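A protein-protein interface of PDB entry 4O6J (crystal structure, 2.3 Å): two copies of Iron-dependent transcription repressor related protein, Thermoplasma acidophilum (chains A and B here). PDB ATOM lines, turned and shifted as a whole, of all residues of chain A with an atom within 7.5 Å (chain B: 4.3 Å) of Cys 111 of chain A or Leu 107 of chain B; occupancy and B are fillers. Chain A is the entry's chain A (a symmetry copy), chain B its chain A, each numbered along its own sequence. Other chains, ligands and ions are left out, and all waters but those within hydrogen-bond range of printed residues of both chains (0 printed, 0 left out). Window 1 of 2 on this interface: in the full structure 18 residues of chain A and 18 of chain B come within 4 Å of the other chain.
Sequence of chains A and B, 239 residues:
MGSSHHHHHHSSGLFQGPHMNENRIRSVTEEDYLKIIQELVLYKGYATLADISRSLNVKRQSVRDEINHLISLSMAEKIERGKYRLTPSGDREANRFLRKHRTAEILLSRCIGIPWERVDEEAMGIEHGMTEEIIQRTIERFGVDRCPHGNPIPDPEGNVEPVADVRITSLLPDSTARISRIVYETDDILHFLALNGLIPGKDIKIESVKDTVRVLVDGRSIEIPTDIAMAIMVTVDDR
Hydrophobic or aromatic side chains of chain A within 4 Å of the printed part of chain B: Leu 107, Ile 112 and Phe 142. Of the 13 printed residues of chain B, 6 touch a printed residue of chain A. Hydrophobic or aromatic side chains of chain B that line the printed part of chain A: Leu 107, Ile 112 and Phe 142.
Leu 107 of chain A touches Ile 112 of chain B, and with the chains exchanged Ile 112 of chain A touches Leu 107 of chain B. Cys 111 of chain A touches its own counterpart, Cys 111 of chain B. Cys 111 of chain A touches Arg 141 of chain B, and with the chains exchanged Arg 141 of chain A touches Cys 111 of chain B. Cys 111 of chain A touches Phe 142 of chain B, and with the chains exchanged Phe 142 of chain A touches Cys 111 of chain B.
Glu 105 of chain A touches none of the printed residues of chain B. Of chain B, only Leu 107 (3.5 Å), Cys 111 (2.1 Å), Arg 141 (3.2 Å) and Phe 142 (3.5 Å) come within 4 Å of Cys 111 of chain A. Printed residues of chain B within 4 Å of Phe 142 of chain A: Cys 111 (3.5 Å). Ile 106 of chain B touches none of the printed residues of chain A. Leu 107 of chain B touches just these residues of chain A: Cys 111 and Ile 112. Of the printed residues of chain A, Ile 112 of chain B touches Leu 107. Of the printed residues of chain A, Thr 138 of chain B touches Ile 112 (3.8 Å). The nearest printed residue of chain A that does not touch Ile 112 of chain B is Phe 142 of chain A (4.1 Å).
Among the printed residues, merely in contact across the chains: Cys 111 of chain A with Phe 142 of chain B, Phe 142 of chain A with Cys 111 of chain B, Cys 111 of chain A with Leu 107 of chain B, Leu 107 of chain A with Cys 111 of chain B, Ile 112 of chain A with Thr 138 of chain B, Ile 112 of chain A with Leu 107 of chain B and Leu 107 of chain A with Ile 112 of chain B.
NE of Arg 141 of chain B sits at hydrogen-bond distance from O of Cys 111 of chain A, at 3.2 Å. O of Cys 111 of chain B sits at hydrogen-bond distance from NE of Arg 141 of chain A, at 3.2 Å. SG of Cys 111 of chain B forms a disulfide with SG of Cys 111 of chain A.
The backbone carbonyl oxygen (O) of Phe 142 of chain A sits at hydrogen-bond distance from the guanidinium group (NH1) of Arg 110 of chain A, 3.5 Å away. The backbone carbonyl oxygen of Phe 142 of chain B lies within hydrogen-bond range of the guanidinium group of Arg 110 of chain B.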
ATOM      1  N   GLU A 105       1.581   4.979  -3.786  1.00  0.00           N
ATOM      2  CA  GLU A 105       2.277   5.388  -4.996  1.00  0.00           C
ATOM      3  C   GLU A 105       3.794   5.457  -4.827  1.00  0.00           C
ATOM      4  O   GLU A 105       4.524   5.048  -5.713  1.00  0.00           O
ATOM      5  CB  GLU A 105       1.788   6.741  -5.466  1.00  0.00           C
ATOM      6  CG  GLU A 105       0.362   6.733  -5.983  1.00  0.00           C
ATOM      7  CD  GLU A 105       0.042   8.010  -6.701  1.00  0.00           C
ATOM      8  OE1 GLU A 105       0.812   8.969  -6.557  1.00  0.00           O
ATOM      9  OE2 GLU A 105      -0.947   8.051  -7.438  1.00  0.00           O
ATOM     10  N   ILE A 106       4.258   6.018  -3.716  1.00  0.00           N
ATOM     11  CA  ILE A 106       5.695   6.096  -3.445  1.00  0.00           C
ATOM     12  C   ILE A 106       6.267   4.688  -3.351  1.00  0.00           C
ATOM     13  O   ILE A 106       7.307   4.376  -3.951  1.00  0.00           O
ATOM     14  CB  ILE A 106       5.976   6.844  -2.153  1.00  0.00           C
ATOM     15  CG1 ILE A 106       5.705   8.332  -2.336  1.00  0.00           C
ATOM     16  CG2 ILE A 106       7.416   6.671  -1.729  1.00  0.00           C
ATOM     17  CD1 ILE A 106       6.710   9.015  -3.254  1.00  0.00           C
ATOM     18  N   LEU A 107       5.567   3.827  -2.618  1.00  0.00           N
ATOM     19  CA  LEU A 107       5.997   2.428  -2.460  1.00  0.00           C
ATOM     20  C   LEU A 107       6.118   1.779  -3.817  1.00  0.00           C
ATOM     21  O   LEU A 107       7.133   1.222  -4.142  1.00  0.00           O
ATOM     22  CB  LEU A 107       5.014   1.654  -1.576  1.00  0.00           C
ATOM     23  CG  LEU A 107       5.319   0.214  -1.162  1.00  0.00           C
ATOM     24  CD1 LEU A 107       6.671   0.109  -0.482  1.00  0.00           C
ATOM     25  CD2 LEU A 107       4.236  -0.274  -0.225  1.00  0.00           C
ATOM     26  N   LEU A 108       5.085   1.901  -4.639  1.00  0.00           N
ATOM     27  CA  LEU A 108       5.076   1.203  -5.920  1.00  0.00           C
ATOM     28  C   LEU A 108       6.088   1.751  -6.923  1.00  0.00           C
ATOM     29  O   LEU A 108       6.699   0.985  -7.670  1.00  0.00           O
ATOM     30  CB  LEU A 108       3.677   1.251  -6.524  1.00  0.00           C
ATOM     31  CG  LEU A 108       2.638   0.455  -5.747  1.00  0.00           C
ATOM     32  CD1 LEU A 108       1.311   0.480  -6.498  1.00  0.00           C
ATOM     33  CD2 LEU A 108       3.148  -1.010  -5.559  1.00  0.00           C
ATOM     34  N   SER A 109       6.281   3.069  -6.950  1.00  0.00           N
ATOM     35  CA  SER A 109       7.199   3.639  -7.931  1.00  0.00           C
ATOM     36  C   SER A 109       8.666   3.527  -7.484  1.00  0.00           C
ATOM     37  O   SER A 109       9.534   3.214  -8.295  1.00  0.00           O
ATOM     38  CB  SER A 109       6.856   5.100  -8.223  1.00  0.00           C
ATOM     39  OG  SER A 109       7.592   5.937  -7.370  1.00  0.00           O
ATOM     40  N   ARG A 110       8.933   3.715  -6.214  1.00  0.00           N
ATOM     41  CA  ARG A 110      10.285   3.633  -5.735  1.00  0.00           C
ATOM     42  C   ARG A 110      10.771   2.231  -5.481  1.00  0.00           C
ATOM     43  O   ARG A 110      11.889   1.956  -5.783  1.00  0.00           O
ATOM     44  CB  ARG A 110      10.508   4.477  -4.500  1.00  0.00           C
ATOM     45  CG  ARG A 110      10.177   5.928  -4.675  1.00  0.00           C
ATOM     46  CD  ARG A 110      11.312   6.701  -5.260  1.00  0.00           C
ATOM     47  NE  ARG A 110      11.501   7.925  -4.536  1.00  0.00           N
ATOM     48  CZ  ARG A 110      12.484   8.122  -3.685  1.00  0.00           C
ATOM     49  NH1 ARG A 110      12.587   9.266  -3.056  1.00  0.00           N
ATOM     50  NH2 ARG A 110      13.368   7.180  -3.480  1.00  0.00           N
ATOM     51  N   CYS A 111       9.955   1.358  -4.925  1.00  0.00           N
ATOM     52  CA  CYS A 111      10.397   0.008  -4.651  1.00  0.00           C
ATOM     53  C   CYS A 111      10.460  -0.844  -5.926  1.00  0.00           C
ATOM     54  O   CYS A 111      11.437  -1.491  -6.143  1.00  0.00           O
ATOM     55  CB  CYS A 111       9.569  -0.649  -3.521  1.00  0.00           C
ATOM     56  SG  CYS A 111      10.008  -2.317  -2.957  1.00  0.00           S
ATOM     57  N   ILE A 112       9.451  -0.818  -6.782  1.00  0.00           N
ATOM     58  CA  ILE A 112       9.426  -1.730  -7.924  1.00  0.00           C
ATOM     59  C   ILE A 112       9.333  -1.198  -9.337  1.00  0.00           C
ATOM     60  O   ILE A 112       9.200  -1.940 -10.261  1.00  0.00           O
ATOM     61  CB  ILE A 112       8.361  -2.818  -7.775  1.00  0.00           C
ATOM     62  CG1 ILE A 112       6.983  -2.235  -7.698  1.00  0.00           C
ATOM     63  CG2 ILE A 112       8.629  -3.671  -6.561  1.00  0.00           C
ATOM     64  CD1 ILE A 112       5.912  -3.224  -8.004  1.00  0.00           C
ATOM     65  N   GLY A 113       9.400   0.097  -9.491  1.00  0.00           N
ATOM     66  CA  GLY A 113       9.538   0.740 -10.781  1.00  0.00           C
ATOM     67  C   GLY A 113       8.271   0.835 -11.604  1.00  0.00           C
ATOM     68  O   GLY A 113       8.331   0.895 -12.821  1.00  0.00           O
ATOM     69  N   ILE A 114       7.116   0.844 -10.950  1.00  0.00           N
ATOM     70  CA  ILE A 114       5.875   1.118 -11.659  1.00  0.00           C
ATOM     71  C   ILE A 114       5.967   2.523 -12.253  1.00  0.00           C
ATOM     72  O   ILE A 114       6.195   3.474 -11.526  1.00  0.00           O
ATOM     73  CB  ILE A 114       4.659   1.031 -10.741  1.00  0.00           C
ATOM     74  CG1 ILE A 114       4.531  -0.374 -10.129  1.00  0.00           C
ATOM     75  CG2 ILE A 114       3.424   1.420 -11.503  1.00  0.00           C
ATOM     76  CD1 ILE A 114       3.891  -1.400 -11.027  1.00  0.00           C
ATOM     77  N   ILE A 126      -3.729  -1.787  -3.483  1.00  0.00           N
ATOM     78  CA  ILE A 126      -3.108  -1.937  -2.174  1.00  0.00           C
ATOM     79  C   ILE A 126      -3.383  -0.809  -1.185  1.00  0.00           C
ATOM     80  O   ILE A 126      -3.077  -0.938   0.000  1.00  0.00           O
ATOM     81  CB  ILE A 126      -1.603  -2.085  -2.303  1.00  0.00           C
ATOM     82  CG1 ILE A 126      -0.982  -0.811  -2.825  1.00  0.00           C
ATOM     83  CG2 ILE A 126      -1.271  -3.263  -3.239  1.00  0.00           C
ATOM     84  CD1 ILE A 126       0.539  -0.704  -2.545  1.00  0.00           C
ATOM     85  N   ARG A 141      11.834   5.414   4.998  1.00  0.00           N
ATOM     86  CA  ARG A 141      12.765   4.673   4.148  1.00  0.00           C
ATOM     87  C   ARG A 141      13.139   5.449   2.882  1.00  0.00           C
ATOM     88  O   ARG A 141      14.294   5.471   2.474  1.00  0.00           O
ATOM     89  CB  ARG A 141      12.159   3.313   3.768  1.00  0.00           C
ATOM     90  CG  ARG A 141      12.794   2.658   2.545  1.00  0.00           C
ATOM     91  CD  ARG A 141      14.169   2.064   2.832  1.00  0.00           C
ATOM     92  NE  ARG A 141      14.613   1.246   1.700  1.00  0.00           N
ATOM     93  CZ  ARG A 141      15.284   1.702   0.639  1.00  0.00           C
ATOM     94  NH1 ARG A 141      15.635   2.988   0.540  1.00  0.00           N
ATOM     95  NH2 ARG A 141      15.619   0.859  -0.330  1.00  0.00           N
ATOM     96  N   PHE A 142      12.164   6.107   2.266  1.00  0.00           N
ATOM     97  CA  PHE A 142      12.464   6.856   1.057  1.00  0.00           C
ATOM     98  C   PHE A 142      12.625   8.363   1.275  1.00  0.00           C
ATOM     99  O   PHE A 142      13.088   9.057   0.377  1.00  0.00           O
ATOM    100  CB  PHE A 142      11.393   6.590   0.001  1.00  0.00           C
ATOM    101  CG  PHE A 142      11.376   5.164  -0.464  1.00  0.00           C
ATOM    102  CD1 PHE A 142      12.449   4.649  -1.187  1.00  0.00           C
ATOM    103  CD2 PHE A 142      10.318   4.328  -0.149  1.00  0.00           C
ATOM    104  CE1 PHE A 142      12.454   3.324  -1.606  1.00  0.00           C
ATOM    105  CE2 PHE A 142      10.318   2.994  -0.564  1.00  0.00           C
ATOM    106  CZ  PHE A 142      11.388   2.502  -1.294  1.00  0.00           C
ATOM    107  N   THR B 103       3.938 -12.575  -2.143  1.00  0.00           N
ATOM    108  CA  THR B 103       4.567 -11.487  -2.859  1.00  0.00           C
ATOM    109  C   THR B 103       4.486 -10.188  -2.071  1.00  0.00           C
ATOM    110  O   THR B 103       5.390  -9.347  -2.128  1.00  0.00           O
ATOM    111  CB  THR B 103       3.918 -11.298  -4.225  1.00  0.00           C
ATOM    112  OG1 THR B 103       4.005 -12.532  -4.954  1.00  0.00           O
ATOM    113  CG2 THR B 103       4.631 -10.231  -5.002  1.00  0.00           C
ATOM    114  N   ALA B 104       3.395 -10.026  -1.332  1.00  0.00           N
ATOM    115  CA  ALA B 104       3.219  -8.837  -0.514  1.00  0.00           C
ATOM    116  C   ALA B 104       4.262  -8.859   0.590  1.00  0.00           C
ATOM    117  O   ALA B 104       4.861  -7.846   0.893  1.00  0.00           O
ATOM    118  CB  ALA B 104       1.823  -8.780   0.074  1.00  0.00           C
ATOM    119  N   GLU B 105       4.468 -10.028   1.194  1.00  0.00           N
ATOM    120  CA  GLU B 105       5.530 -10.174   2.176  1.00  0.00           C
ATOM    121  C   GLU B 105       6.911  -9.810   1.633  1.00  0.00           C
ATOM    122  O   GLU B 105       7.689  -9.175   2.324  1.00  0.00           O
ATOM    123  CB  GLU B 105       5.585 -11.592   2.702  1.00  0.00           C
ATOM    124  CG  GLU B 105       4.392 -11.975   3.558  1.00  0.00           C
ATOM    125  CD  GLU B 105       4.641 -13.263   4.285  1.00  0.00           C
ATOM    126  OE1 GLU B 105       5.594 -13.965   3.919  1.00  0.00           O
ATOM    127  OE2 GLU B 105       3.922 -13.559   5.242  1.00  0.00           O
ATOM    128  N   ILE B 106       7.226 -10.255   0.422  1.00  0.00           N
ATOM    129  CA  ILE B 106       8.510  -9.925  -0.200  1.00  0.00           C
ATOM    130  C   ILE B 106       8.611  -8.417  -0.382  1.00  0.00           C
ATOM    131  O   ILE B 106       9.631  -7.797  -0.048  1.00  0.00           O
ATOM    132  CB  ILE B 106       8.664 -10.608  -1.549  1.00  0.00           C
ATOM    133  CG1 ILE B 106       8.887 -12.103  -1.359  1.00  0.00           C
ATOM    134  CG2 ILE B 106       9.840 -10.044  -2.310  1.00  0.00           C
ATOM    135  CD1 ILE B 106      10.241 -12.433  -0.746  1.00  0.00           C
ATOM    136  N   LEU B 107       7.533  -7.821  -0.885  1.00  0.00           N
ATOM    137  CA  LEU B 107       7.488  -6.365  -1.093  1.00  0.00           C
ATOM    138  C   LEU B 107       7.751  -5.659   0.215  1.00  0.00           C
ATOM    139  O   LEU B 107       8.610  -4.821   0.297  1.00  0.00           O
ATOM    140  CB  LEU B 107       6.136  -5.940  -1.675  1.00  0.00           C
ATOM    141  CG  LEU B 107       5.901  -4.490  -2.099  1.00  0.00           C
ATOM    142  CD1 LEU B 107       6.953  -4.025  -3.089  1.00  0.00           C
ATOM    143  CD2 LEU B 107       4.526  -4.369  -2.717  1.00  0.00           C
ATOM    144  N   LEU B 108       7.035  -6.043   1.262  1.00  0.00           N
ATOM    145  CA  LEU B 108       7.144  -5.329   2.530  1.00  0.00           C
ATOM    146  C   LEU B 108       8.487  -5.525   3.230  1.00  0.00           C
ATOM    147  O   LEU B 108       9.017  -4.589   3.829  1.00  0.00           O
ATOM    148  CB  LEU B 108       6.015  -5.756   3.462  1.00  0.00           C
ATOM    149  CG  LEU B 108       4.631  -5.322   2.997  1.00  0.00           C
ATOM    150  CD1 LEU B 108       3.598  -5.699   4.053  1.00  0.00           C
ATOM    151  CD2 LEU B 108       4.635  -3.779   2.743  1.00  0.00           C
ATOM    152  N   SER B 109       9.052  -6.730   3.158  1.00  0.00           N
ATOM    153  CA  SER B 109      10.308  -6.974   3.858  1.00  0.00           C
ATOM    154  C   SER B 109      11.522  -6.462   3.066  1.00  0.00           C
ATOM    155  O   SER B 109      12.436  -5.882   3.646  1.00  0.00           O
ATOM    156  CB  SER B 109      10.484  -8.460   4.173  1.00  0.00           C
ATOM    157  OG  SER B 109      11.194  -9.081   3.132  1.00  0.00           O
ATOM    158  N   ARG B 110      11.507  -6.612   1.763  1.00  0.00           N
ATOM    159  CA  ARG B 110      12.616  -6.162   0.967  1.00  0.00           C
ATOM    160  C   ARG B 110      12.598  -4.690   0.652  1.00  0.00           C
ATOM    161  O   ARG B 110      13.628  -4.094   0.677  1.00  0.00           O
ATOM    162  CB  ARG B 110      12.757  -6.951  -0.316  1.00  0.00           C
ATOM    163  CG  ARG B 110      12.912  -8.429  -0.118  1.00  0.00           C
ATOM    164  CD  ARG B 110      14.330  -8.820   0.138  1.00  0.00           C
ATOM    165  NE  ARG B 110      14.677  -9.964  -0.656  1.00  0.00           N
ATOM    166  CZ  ARG B 110      15.432  -9.901  -1.731  1.00  0.00           C
ATOM    167  NH1 ARG B 110      15.700 -10.990  -2.408  1.00  0.00           N
ATOM    168  NH2 ARG B 110      15.927  -8.753  -2.115  1.00  0.00           N
ATOM    169  N   CYS B 111      11.453  -4.110   0.349  1.00  0.00           N
ATOM    170  CA  CYS B 111      11.405  -2.701   0.024  1.00  0.00           C
ATOM    171  C   CYS B 111      11.536  -1.820   1.275  1.00  0.00           C
ATOM    172  O   CYS B 111      12.307  -0.912   1.266  1.00  0.00           O
ATOM    173  CB  CYS B 111      10.170  -2.352  -0.840  1.00  0.00           C
ATOM    174  SG  CYS B 111       9.956  -0.652  -1.433  1.00  0.00           S
ATOM    175  N   ILE B 112      10.823  -2.104   2.353  1.00  0.00           N
ATOM    176  CA  ILE B 112      10.821  -1.196   3.498  1.00  0.00           C
ATOM    177  C   ILE B 112      11.239  -1.679   4.869  1.00  0.00           C
ATOM    178  O   ILE B 112      11.133  -0.973   5.824  1.00  0.00           O
ATOM    179  CB  ILE B 112       9.486  -0.467   3.659  1.00  0.00           C
ATOM    180  CG1 ILE B 112       8.360  -1.424   3.905  1.00  0.00           C
ATOM    181  CG2 ILE B 112       9.186   0.382   2.449  1.00  0.00           C
ATOM    182  CD1 ILE B 112       7.161  -0.774   4.505  1.00  0.00           C
ATOM    183  N   THR B 138       7.293  -7.179  -8.794  1.00  0.00           N
ATOM    184  CA  THR B 138       7.945  -7.453  -7.514  1.00  0.00           C
ATOM    185  C   THR B 138       8.852  -8.697  -7.627  1.00  0.00           C
ATOM    186  O   THR B 138       9.987  -8.717  -7.151  1.00  0.00           O
ATOM    187  CB  THR B 138       6.907  -7.688  -6.383  1.00  0.00           C
ATOM    188  OG1 THR B 138       6.135  -6.506  -6.186  1.00  0.00           O
ATOM    189  CG2 THR B 138       7.587  -8.061  -5.064  1.00  0.00           C
ATOM    190  N   ARG B 141      11.893  -7.819  -9.873  1.00  0.00           N
ATOM    191  CA  ARG B 141      12.751  -6.811  -9.255  1.00  0.00           C
ATOM    192  C   ARG B 141      13.635  -7.398  -8.151  1.00  0.00           C
ATOM    193  O   ARG B 141      14.811  -7.072  -8.043  1.00  0.00           O
ATOM    194  CB  ARG B 141      11.894  -5.670  -8.685  1.00  0.00           C
ATOM    195  CG  ARG B 141      12.597  -4.815  -7.635  1.00  0.00           C
ATOM    196  CD  ARG B 141      13.626  -3.861  -8.232  1.00  0.00           C
ATOM    197  NE  ARG B 141      14.082  -2.908  -7.217  1.00  0.00           N
ATOM    198  CZ  ARG B 141      15.098  -3.112  -6.374  1.00  0.00           C
ATOM    199  NH1 ARG B 141      15.818  -4.238  -6.414  1.00  0.00           N
ATOM    200  NH2 ARG B 141      15.407  -2.173  -5.488  1.00  0.00           N
ATOM    201  N   PHE B 142      13.076  -8.286  -7.336  1.00  0.00           N
ATOM    202  CA  PHE B 142      13.870  -8.871  -6.269  1.00  0.00           C
ATOM    203  C   PHE B 142      14.398 -10.276  -6.576  1.00  0.00           C
ATOM    204  O   PHE B 142      15.250 -10.773  -5.848  1.00  0.00           O
ATOM    205  CB  PHE B 142      13.065  -8.886  -4.971  1.00  0.00           C
ATOM    206  CG  PHE B 142      12.755  -7.509  -4.463  1.00  0.00           C
ATOM    207  CD1 PHE B 142      13.778  -6.681  -4.011  1.00  0.00           C
ATOM    208  CD2 PHE B 142      11.457  -7.026  -4.475  1.00  0.00           C
ATOM    209  CE1 PHE B 142      13.506  -5.395  -3.557  1.00  0.00           C
ATOM    210  CE2 PHE B 142      11.176  -5.733  -4.023  1.00  0.00           C
ATOM    211  CZ  PHE B 142      12.206  -4.927  -3.564  1.00  0.00           C
